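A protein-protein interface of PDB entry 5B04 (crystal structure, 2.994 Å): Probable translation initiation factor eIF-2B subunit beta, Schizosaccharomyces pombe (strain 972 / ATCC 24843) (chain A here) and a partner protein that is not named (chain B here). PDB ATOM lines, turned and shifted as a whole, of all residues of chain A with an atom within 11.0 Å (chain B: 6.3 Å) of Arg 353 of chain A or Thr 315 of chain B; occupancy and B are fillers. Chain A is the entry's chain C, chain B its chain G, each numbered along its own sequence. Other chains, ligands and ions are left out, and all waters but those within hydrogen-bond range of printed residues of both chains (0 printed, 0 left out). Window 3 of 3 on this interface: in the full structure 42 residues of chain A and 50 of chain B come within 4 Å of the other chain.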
ATOM      1  N   MET A 343      -2.138  -8.532  23.842  1.00  0.00           N
ATOM      2  CA  MET A 343      -2.425  -7.117  24.040  1.00  0.00           C
ATOM      3  C   MET A 343      -3.911  -6.910  24.309  1.00  0.00           C
ATOM      4  O   MET A 343      -4.760  -7.502  23.643  1.00  0.00           O
ATOM      5  CB  MET A 343      -1.987  -6.303  22.821  1.00  0.00           C
ATOM      6  CG  MET A 343      -2.336  -4.824  22.895  1.00  0.00           C
ATOM      7  SD  MET A 343      -1.406  -3.936  24.158  1.00  0.00           S
ATOM      8  CE  MET A 343       0.243  -3.999  23.466  1.00  0.00           C
ATOM      9  N   SER A 344      -4.220  -6.071  25.292  1.00  0.00           N
ATOM     10  CA  SER A 344      -5.605  -5.804  25.653  1.00  0.00           C
ATOM     11  C   SER A 344      -6.298  -4.970  24.581  1.00  0.00           C
ATOM     12  O   SER A 344      -5.669  -4.142  23.922  1.00  0.00           O
ATOM     13  CB  SER A 344      -5.679  -5.100  27.006  1.00  0.00           C
ATOM     14  OG  SER A 344      -7.026  -4.917  27.405  1.00  0.00           O
ATOM     15  N   PHE A 345      -7.596  -5.192  24.413  1.00  0.00           N
ATOM     16  CA  PHE A 345      -8.357  -4.535  23.358  1.00  0.00           C
ATOM     17  C   PHE A 345      -8.654  -3.074  23.683  1.00  0.00           C
ATOM     18  O   PHE A 345      -8.832  -2.259  22.778  1.00  0.00           O
ATOM     19  CB  PHE A 345      -9.661  -5.290  23.100  1.00  0.00           C
ATOM     20  CG  PHE A 345     -10.469  -4.738  21.960  1.00  0.00           C
ATOM     21  CD1 PHE A 345     -10.116  -5.011  20.648  1.00  0.00           C
ATOM     22  CD2 PHE A 345     -11.585  -3.956  22.199  1.00  0.00           C
ATOM     23  CE1 PHE A 345     -10.859  -4.508  19.596  1.00  0.00           C
ATOM     24  CE2 PHE A 345     -12.332  -3.449  21.152  1.00  0.00           C
ATOM     25  CZ  PHE A 345     -11.968  -3.727  19.849  1.00  0.00           C
ATOM     26  N   GLU A 347      -6.668  -1.041  24.688  1.00  0.00           N
ATOM     27  CA  GLU A 347      -5.515  -0.270  24.238  1.00  0.00           C
ATOM     28  C   GLU A 347      -5.699   0.125  22.777  1.00  0.00           C
ATOM     29  O   GLU A 347      -5.020  -0.399  21.892  1.00  0.00           O
ATOM     30  CB  GLU A 347      -4.222  -1.068  24.417  1.00  0.00           C
ATOM     31  CG  GLU A 347      -3.715  -1.126  25.848  1.00  0.00           C
ATOM     32  CD  GLU A 347      -3.095   0.183  26.297  1.00  0.00           C
ATOM     33  OE1 GLU A 347      -2.963   0.392  27.522  1.00  0.00           O
ATOM     34  OE2 GLU A 347      -2.732   1.001  25.425  1.00  0.00           O
ATOM     35  N   GLY A 348      -6.622   1.052  22.538  1.00  0.00           N
ATOM     36  CA  GLY A 348      -7.000   1.445  21.192  1.00  0.00           C
ATOM     37  C   GLY A 348      -5.870   1.985  20.337  1.00  0.00           C
ATOM     38  O   GLY A 348      -5.714   1.584  19.185  1.00  0.00           O
ATOM     39  N   ASP A 349      -5.084   2.898  20.897  1.00  0.00           N
ATOM     40  CA  ASP A 349      -3.996   3.524  20.153  1.00  0.00           C
ATOM     41  C   ASP A 349      -2.911   2.521  19.775  1.00  0.00           C
ATOM     42  O   ASP A 349      -2.372   2.569  18.670  1.00  0.00           O
ATOM     43  CB  ASP A 349      -3.383   4.671  20.961  1.00  0.00           C
ATOM     44  CG  ASP A 349      -4.318   5.856  21.092  1.00  0.00           C
ATOM     45  OD1 ASP A 349      -5.220   6.000  20.240  1.00  0.00           O
ATOM     46  OD2 ASP A 349      -4.147   6.646  22.044  1.00  0.00           O
ATOM     47  N   LEU A 350      -2.597   1.614  20.693  1.00  0.00           N
ATOM     48  CA  LEU A 350      -1.532   0.643  20.465  1.00  0.00           C
ATOM     49  C   LEU A 350      -1.892  -0.355  19.370  1.00  0.00           C
ATOM     50  O   LEU A 350      -1.103  -0.590  18.454  1.00  0.00           O
ATOM     51  CB  LEU A 350      -1.198  -0.102  21.759  1.00  0.00           C
ATOM     52  CG  LEU A 350      -0.571   0.730  22.878  1.00  0.00           C
ATOM     53  CD1 LEU A 350       0.102  -0.171  23.903  1.00  0.00           C
ATOM     54  CD2 LEU A 350       0.417   1.739  22.314  1.00  0.00           C
ATOM     55  N   ILE A 351      -3.083  -0.936  19.462  1.00  0.00           N
ATOM     56  CA  ILE A 351      -3.507  -1.956  18.510  1.00  0.00           C
ATOM     57  C   ILE A 351      -3.741  -1.373  17.118  1.00  0.00           C
ATOM     58  O   ILE A 351      -3.717  -2.095  16.122  1.00  0.00           O
ATOM     59  CB  ILE A 351      -4.791  -2.670  18.982  1.00  0.00           C
ATOM     60  CG1 ILE A 351      -5.975  -1.699  19.002  1.00  0.00           C
ATOM     61  CG2 ILE A 351      -4.578  -3.286  20.355  1.00  0.00           C
ATOM     62  CD1 ILE A 351      -7.271  -2.330  19.459  1.00  0.00           C
ATOM     63  N   SER A 352      -3.959  -0.063  17.054  1.00  0.00           N
ATOM     64  CA  SER A 352      -4.184   0.612  15.783  1.00  0.00           C
ATOM     65  C   SER A 352      -2.865   0.957  15.102  1.00  0.00           C
ATOM     66  O   SER A 352      -2.814   1.148  13.887  1.00  0.00           O
ATOM     67  CB  SER A 352      -5.015   1.880  15.990  1.00  0.00           C
ATOM     68  OG  SER A 352      -4.367   2.774  16.878  1.00  0.00           O
ATOM     69  N   ARG A 353      -1.799   1.028  15.893  1.00  0.00           N
ATOM     70  CA  ARG A 353      -0.501   1.459  15.390  1.00  0.00           C
ATOM     71  C   ARG A 353       0.555   0.362  15.465  1.00  0.00           C
ATOM     72  O   ARG A 353       1.743   0.625  15.278  1.00  0.00           O
ATOM     73  CB  ARG A 353      -0.020   2.685  16.168  1.00  0.00           C
ATOM     74  CG  ARG A 353      -0.936   3.889  16.061  1.00  0.00           C
ATOM     75  CD  ARG A 353      -0.593   4.925  17.115  1.00  0.00           C
ATOM     76  NE  ARG A 353      -1.463   6.094  17.041  1.00  0.00           N
ATOM     77  CZ  ARG A 353      -1.527   7.036  17.975  1.00  0.00           C
ATOM     78  NH1 ARG A 353      -0.775   6.945  19.063  1.00  0.00           N
ATOM     79  NH2 ARG A 353      -2.347   8.067  17.825  1.00  0.00           N
ATOM     80  N   ALA A 354       0.128  -0.865  15.739  1.00  0.00           N
ATOM     81  CA  ALA A 354       1.071  -1.969  15.869  1.00  0.00           C
ATOM     82  C   ALA A 354       0.485  -3.298  15.407  1.00  0.00           C
ATOM     83  O   ALA A 354      -0.724  -3.520  15.473  1.00  0.00           O
ATOM     84  CB  ALA A 354       1.550  -2.082  17.308  1.00  0.00           C
ATOM     85  N   GLU A 355       1.363  -4.177  14.939  1.00  0.00           N
ATOM     86  CA  GLU A 355       0.986  -5.527  14.550  1.00  0.00           C
ATOM     87  C   GLU A 355       1.151  -6.468  15.738  1.00  0.00           C
ATOM     88  O   GLU A 355       2.265  -6.678  16.217  1.00  0.00           O
ATOM     89  CB  GLU A 355       1.837  -5.996  13.368  1.00  0.00           C
ATOM     90  CG  GLU A 355       1.574  -7.421  12.918  1.00  0.00           C
ATOM     91  CD  GLU A 355       2.331  -7.771  11.649  1.00  0.00           C
ATOM     92  OE1 GLU A 355       1.797  -7.515  10.551  1.00  0.00           O
ATOM     93  OE2 GLU A 355       3.461  -8.294  11.751  1.00  0.00           O
ATOM     94  N   ILE A 356       0.045  -7.022  16.221  1.00  0.00           N
ATOM     95  CA  ILE A 356       0.096  -7.920  17.370  1.00  0.00           C
ATOM     96  C   ILE A 356      -0.141  -9.361  16.934  1.00  0.00           C
ATOM     97  O   ILE A 356      -1.160  -9.675  16.320  1.00  0.00           O
ATOM     98  CB  ILE A 356      -0.932  -7.537  18.455  1.00  0.00           C
ATOM     99  CG1 ILE A 356      -0.572  -6.192  19.095  1.00  0.00           C
ATOM    100  CG2 ILE A 356      -0.976  -8.600  19.534  1.00  0.00           C
ATOM    101  CD1 ILE A 356      -1.108  -4.978  18.363  1.00  0.00           C
ATOM    102  N   LEU A 357       0.809 -10.234  17.257  1.00  0.00           N
ATOM    103  CA  LEU A 357       0.779 -11.612  16.782  1.00  0.00           C
ATOM    104  C   LEU A 357       0.823 -12.620  17.926  1.00  0.00           C
ATOM    105  O   LEU A 357       1.749 -12.616  18.734  1.00  0.00           O
ATOM    106  CB  LEU A 357       1.948 -11.860  15.830  1.00  0.00           C
ATOM    107  CG  LEU A 357       2.060 -10.879  14.661  1.00  0.00           C
ATOM    108  CD1 LEU A 357       3.343 -11.114  13.879  1.00  0.00           C
ATOM    109  CD2 LEU A 357       0.846 -10.994  13.754  1.00  0.00           C
ATOM    110  N   CYS B 310       7.463   0.484  25.830  1.00  0.00           N
ATOM    111  CA  CYS B 310       8.290   0.620  24.639  1.00  0.00           C
ATOM    112  C   CYS B 310       7.424   0.811  23.399  1.00  0.00           C
ATOM    113  O   CYS B 310       7.618   1.761  22.639  1.00  0.00           O
ATOM    114  CB  CYS B 310       9.190  -0.605  24.470  1.00  0.00           C
ATOM    115  SG  CYS B 310      10.117  -0.641  22.919  1.00  0.00           S
ATOM    116  N   LEU B 311       6.471  -0.097  23.206  1.00  0.00           N
ATOM    117  CA  LEU B 311       5.564  -0.043  22.063  1.00  0.00           C
ATOM    118  C   LEU B 311       4.799   1.274  22.022  1.00  0.00           C
ATOM    119  O   LEU B 311       4.608   1.861  20.958  1.00  0.00           O
ATOM    120  CB  LEU B 311       4.581  -1.214  22.100  1.00  0.00           C
ATOM    121  CG  LEU B 311       3.595  -1.276  20.933  1.00  0.00           C
ATOM    122  CD1 LEU B 311       4.342  -1.460  19.626  1.00  0.00           C
ATOM    123  CD2 LEU B 311       2.578  -2.384  21.131  1.00  0.00           C
ATOM    124  N   LYS B 312       4.362   1.729  23.193  1.00  0.00           N
ATOM    125  CA  LYS B 312       3.677   3.008  23.314  1.00  0.00           C
ATOM    126  C   LYS B 312       4.572   4.142  22.830  1.00  0.00           C
ATOM    127  O   LYS B 312       4.168   4.954  21.999  1.00  0.00           O
ATOM    128  CB  LYS B 312       3.251   3.252  24.763  1.00  0.00           C
ATOM    129  CG  LYS B 312       2.475   4.539  24.982  1.00  0.00           C
ATOM    130  CD  LYS B 312       2.206   4.769  26.460  1.00  0.00           C
ATOM    131  CE  LYS B 312       1.404   6.040  26.683  1.00  0.00           C
ATOM    132  NZ  LYS B 312       2.073   7.228  26.083  1.00  0.00           N
ATOM    133  N   LEU B 313       5.794   4.177  23.349  1.00  0.00           N
ATOM    134  CA  LEU B 313       6.762   5.208  22.999  1.00  0.00           C
ATOM    135  C   LEU B 313       7.097   5.218  21.510  1.00  0.00           C
ATOM    136  O   LEU B 313       7.035   6.260  20.859  1.00  0.00           O
ATOM    137  CB  LEU B 313       8.043   5.023  23.816  1.00  0.00           C
ATOM    138  CG  LEU B 313       9.250   5.881  23.426  1.00  0.00           C
ATOM    139  CD1 LEU B 313       8.945   7.361  23.597  1.00  0.00           C
ATOM    140  CD2 LEU B 313      10.474   5.484  24.238  1.00  0.00           C
ATOM    141  N   LEU B 314       7.447   4.052  20.976  1.00  0.00           N
ATOM    142  CA  LEU B 314       7.932   3.954  19.603  1.00  0.00           C
ATOM    143  C   LEU B 314       6.857   4.258  18.561  1.00  0.00           C
ATOM    144  O   LEU B 314       7.162   4.766  17.483  1.00  0.00           O
ATOM    145  CB  LEU B 314       8.520   2.565  19.347  1.00  0.00           C
ATOM    146  CG  LEU B 314       9.740   2.189  20.190  1.00  0.00           C
ATOM    147  CD1 LEU B 314      10.381   0.913  19.667  1.00  0.00           C
ATOM    148  CD2 LEU B 314      10.749   3.328  20.224  1.00  0.00           C
ATOM    149  N   THR B 315       5.605   3.947  18.879  1.00  0.00           N
ATOM    150  CA  THR B 315       4.510   4.210  17.950  1.00  0.00           C
ATOM    151  C   THR B 315       4.074   5.670  18.011  1.00  0.00           C
ATOM    152  O   THR B 315       3.474   6.186  17.069  1.00  0.00           O
ATOM    153  CB  THR B 315       3.295   3.305  18.227  1.00  0.00           C
ATOM    154  OG1 THR B 315       2.931   3.397  19.610  1.00  0.00           O
ATOM    155  CG2 THR B 315       3.618   1.858  17.884  1.00  0.00           C
ATOM    156  N   GLU B 316       4.376   6.331  19.124  1.00  0.00           N
ATOM    157  CA  GLU B 316       4.080   7.753  19.267  1.00  0.00           C
ATOM    158  C   GLU B 316       5.110   8.591  18.517  1.00  0.00           C
ATOM    159  O   GLU B 316       4.883   9.769  18.241  1.00  0.00           O
ATOM    160  CB  GLU B 316       4.038   8.152  20.744  1.00  0.00           C
ATOM    161  CG  GLU B 316       2.762   7.736  21.458  1.00  0.00           C
ATOM    162  CD  GLU B 316       2.786   8.065  22.939  1.00  0.00           C
ATOM    163  OE1 GLU B 316       3.872   8.402  23.456  1.00  0.00           O
ATOM    164  OE2 GLU B 316       1.720   7.986  23.586  1.00  0.00           O
ATOM    165  N   HIS B 317       6.242   7.976  18.192  1.00  0.00           N
ATOM    166  CA  HIS B 317       7.253   8.620  17.363  1.00  0.00           C
ATOM    167  C   HIS B 317       7.098   8.185  15.912  1.00  0.00           C
ATOM    168  O   HIS B 317       7.957   8.457  15.072  1.00  0.00           O
ATOM    169  CB  HIS B 317       8.660   8.303  17.872  1.00  0.00           C
ATOM    170  CG  HIS B 317       9.052   9.084  19.088  1.00  0.00           C
ATOM    171  ND1 HIS B 317       9.959  10.119  19.045  1.00  0.00           N
ATOM    172  CD2 HIS B 317       8.654   8.985  20.378  1.00  0.00           C
ATOM    173  CE1 HIS B 317      10.108  10.622  20.258  1.00  0.00           C
ATOM    174  NE2 HIS B 317       9.326   9.951  21.085  1.00  0.00           N
ATOM    175  N   GLY B 318       5.994   7.501  15.629  1.00  0.00           N
ATOM    176  CA  GLY B 318       5.650   7.119  14.272  1.00  0.00           C
ATOM    177  C   GLY B 318       6.550   6.062  13.661  1.00  0.00           C
ATOM    178  O   GLY B 318       6.881   6.133  12.478  1.00  0.00           O
ATOM    179  N   ILE B 319       6.943   5.077  14.462  1.00  0.00           N
ATOM    180  CA  ILE B 319       7.759   3.978  13.963  1.00  0.00           C
ATOM    181  C   ILE B 319       6.911   2.723  13.771  1.00  0.00           C
ATOM    182  O   ILE B 319       6.097   2.378  14.628  1.00  0.00           O
ATOM    183  CB  ILE B 319       8.932   3.660  14.911  1.00  0.00           C
ATOM    184  CG1 ILE B 319       9.669   4.943  15.299  1.00  0.00           C
ATOM    185  CG2 ILE B 319       9.888   2.668  14.266  1.00  0.00           C
ATOM    186  CD1 ILE B 319      10.856   4.713  16.210  1.00  0.00           C
ATOM    187  N   GLU B 320       7.099   2.054  12.639  1.00  0.00           N
ATOM    188  CA  GLU B 320       6.390   0.813  12.344  1.00  0.00           C
ATOM    189  C   GLU B 320       6.799  -0.275  13.333  1.00  0.00           C
ATOM    190  O   GLU B 320       7.985  -0.565  13.488  1.00  0.00           O
ATOM    191  CB  GLU B 320       6.671   0.371  10.906  1.00  0.00           C
ATOM    192  CG  GLU B 320       5.878  -0.839  10.446  1.00  0.00           C
ATOM    193  CD  GLU B 320       6.078  -1.131   8.971  1.00  0.00           C
ATOM    194  OE1 GLU B 320       5.578  -2.172   8.495  1.00  0.00           O
ATOM    195  OE2 GLU B 320       6.736  -0.318   8.287  1.00  0.00           O
ATOM    196  N   CYS B 321       5.820  -0.875  14.005  1.00  0.00           N
ATOM    197  CA  CYS B 321       6.121  -1.802  15.091  1.00  0.00           C
ATOM    198  C   CYS B 321       5.299  -3.089  15.076  1.00  0.00           C
ATOM    199  O   CYS B 321       4.119  -3.091  14.724  1.00  0.00           O
ATOM    200  CB  CYS B 321       5.926  -1.102  16.437  1.00  0.00           C
ATOM    201  SG  CYS B 321       7.151   0.169  16.813  1.00  0.00           S
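Met 343 of chain A touches Leu 311 of chain B (CE to CD2, 3.7 Å).
Lys 312 of chain B touches Leu 350 of chain A.
Arg 353 of chain A touches Thr 315 of chain B (O to CG2, 3.4 Å).
CD1 of Leu 311 of chain B touches CB of Ala 354 of chain A, 3.7 Å away.
Cys 321 of chain B touches Ala 354 of chain A (O to CA, 3.4 Å).
Hydrophobic or aromatic side chains of chain B that line the printed part of chain A: Leu 311.
Of the 14 printed residues of chain A, 5 touch a printed residue of chain B.
Hydrophobic or aromatic side chains of chain A within 4 Å of the printed part of chain B: Met 343, Leu 350 and Ala 354.
Printed residues of chain B within 4 Å of Met 343 of chain A: Leu 311 (3.7 Å).
Ser 352 of chain A touches none of the printed residues of chain B.
Arg 353 of chain A touches just one residue of chain B: Thr 315.
Printed residues of chain B within 4 Å of Glu 355 of chain A: Cys 321 (3.0 Å).
Printed residues of chain A within 4 Å of Lys 312 of chain B: Leu 350.
Of the printed residues of chain A, Thr 315 of chain B touches Arg 353 (3.4 Å).
No residue of chain A comes within 4 Å of Gly 318 of chain B.
No residue of chain A comes within 4 Å of Ile 319 of chain B.
Of chain A, only Ala 354 and Glu 355 come within 4 Å of Cys 321 of chain B.
The nearest residue of chain A that does not touch Thr 315 of chain B is Leu 350 of chain A (4.05 Å).
The nearest printed residue of chain B that does not touch Leu 350 of chain A is Thr 315 of chain B (4.05 Å).
The backbone carbonyl oxygen (O) of Cys 321 of chain B lies within hydrogen-bond range of the backbone NH (N) of Glu 355 of chain A (3.0 Å).
The side-chain hydroxyl (OG1) of Thr 315 of chain B sits at hydrogen-bond distance from the backbone carbonyl oxygen (O) of Leu 311 of chain B (2.6 Å).
The side-chain hydroxyl of Thr 315 of chain B lies within hydrogen-bond range of the backbone carbonyl oxygen of Lys 312 of chain B.
NZ of Lys 312 of chain B is in salt-bridge range of OE2 of Glu 316 of chain B.
The backbone carbonyl oxygen (O) of Ile 319 of chain B lies within hydrogen-bond range of the side-chain sulfur (SG) of Cys 321 of chain B (3.3 Å).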
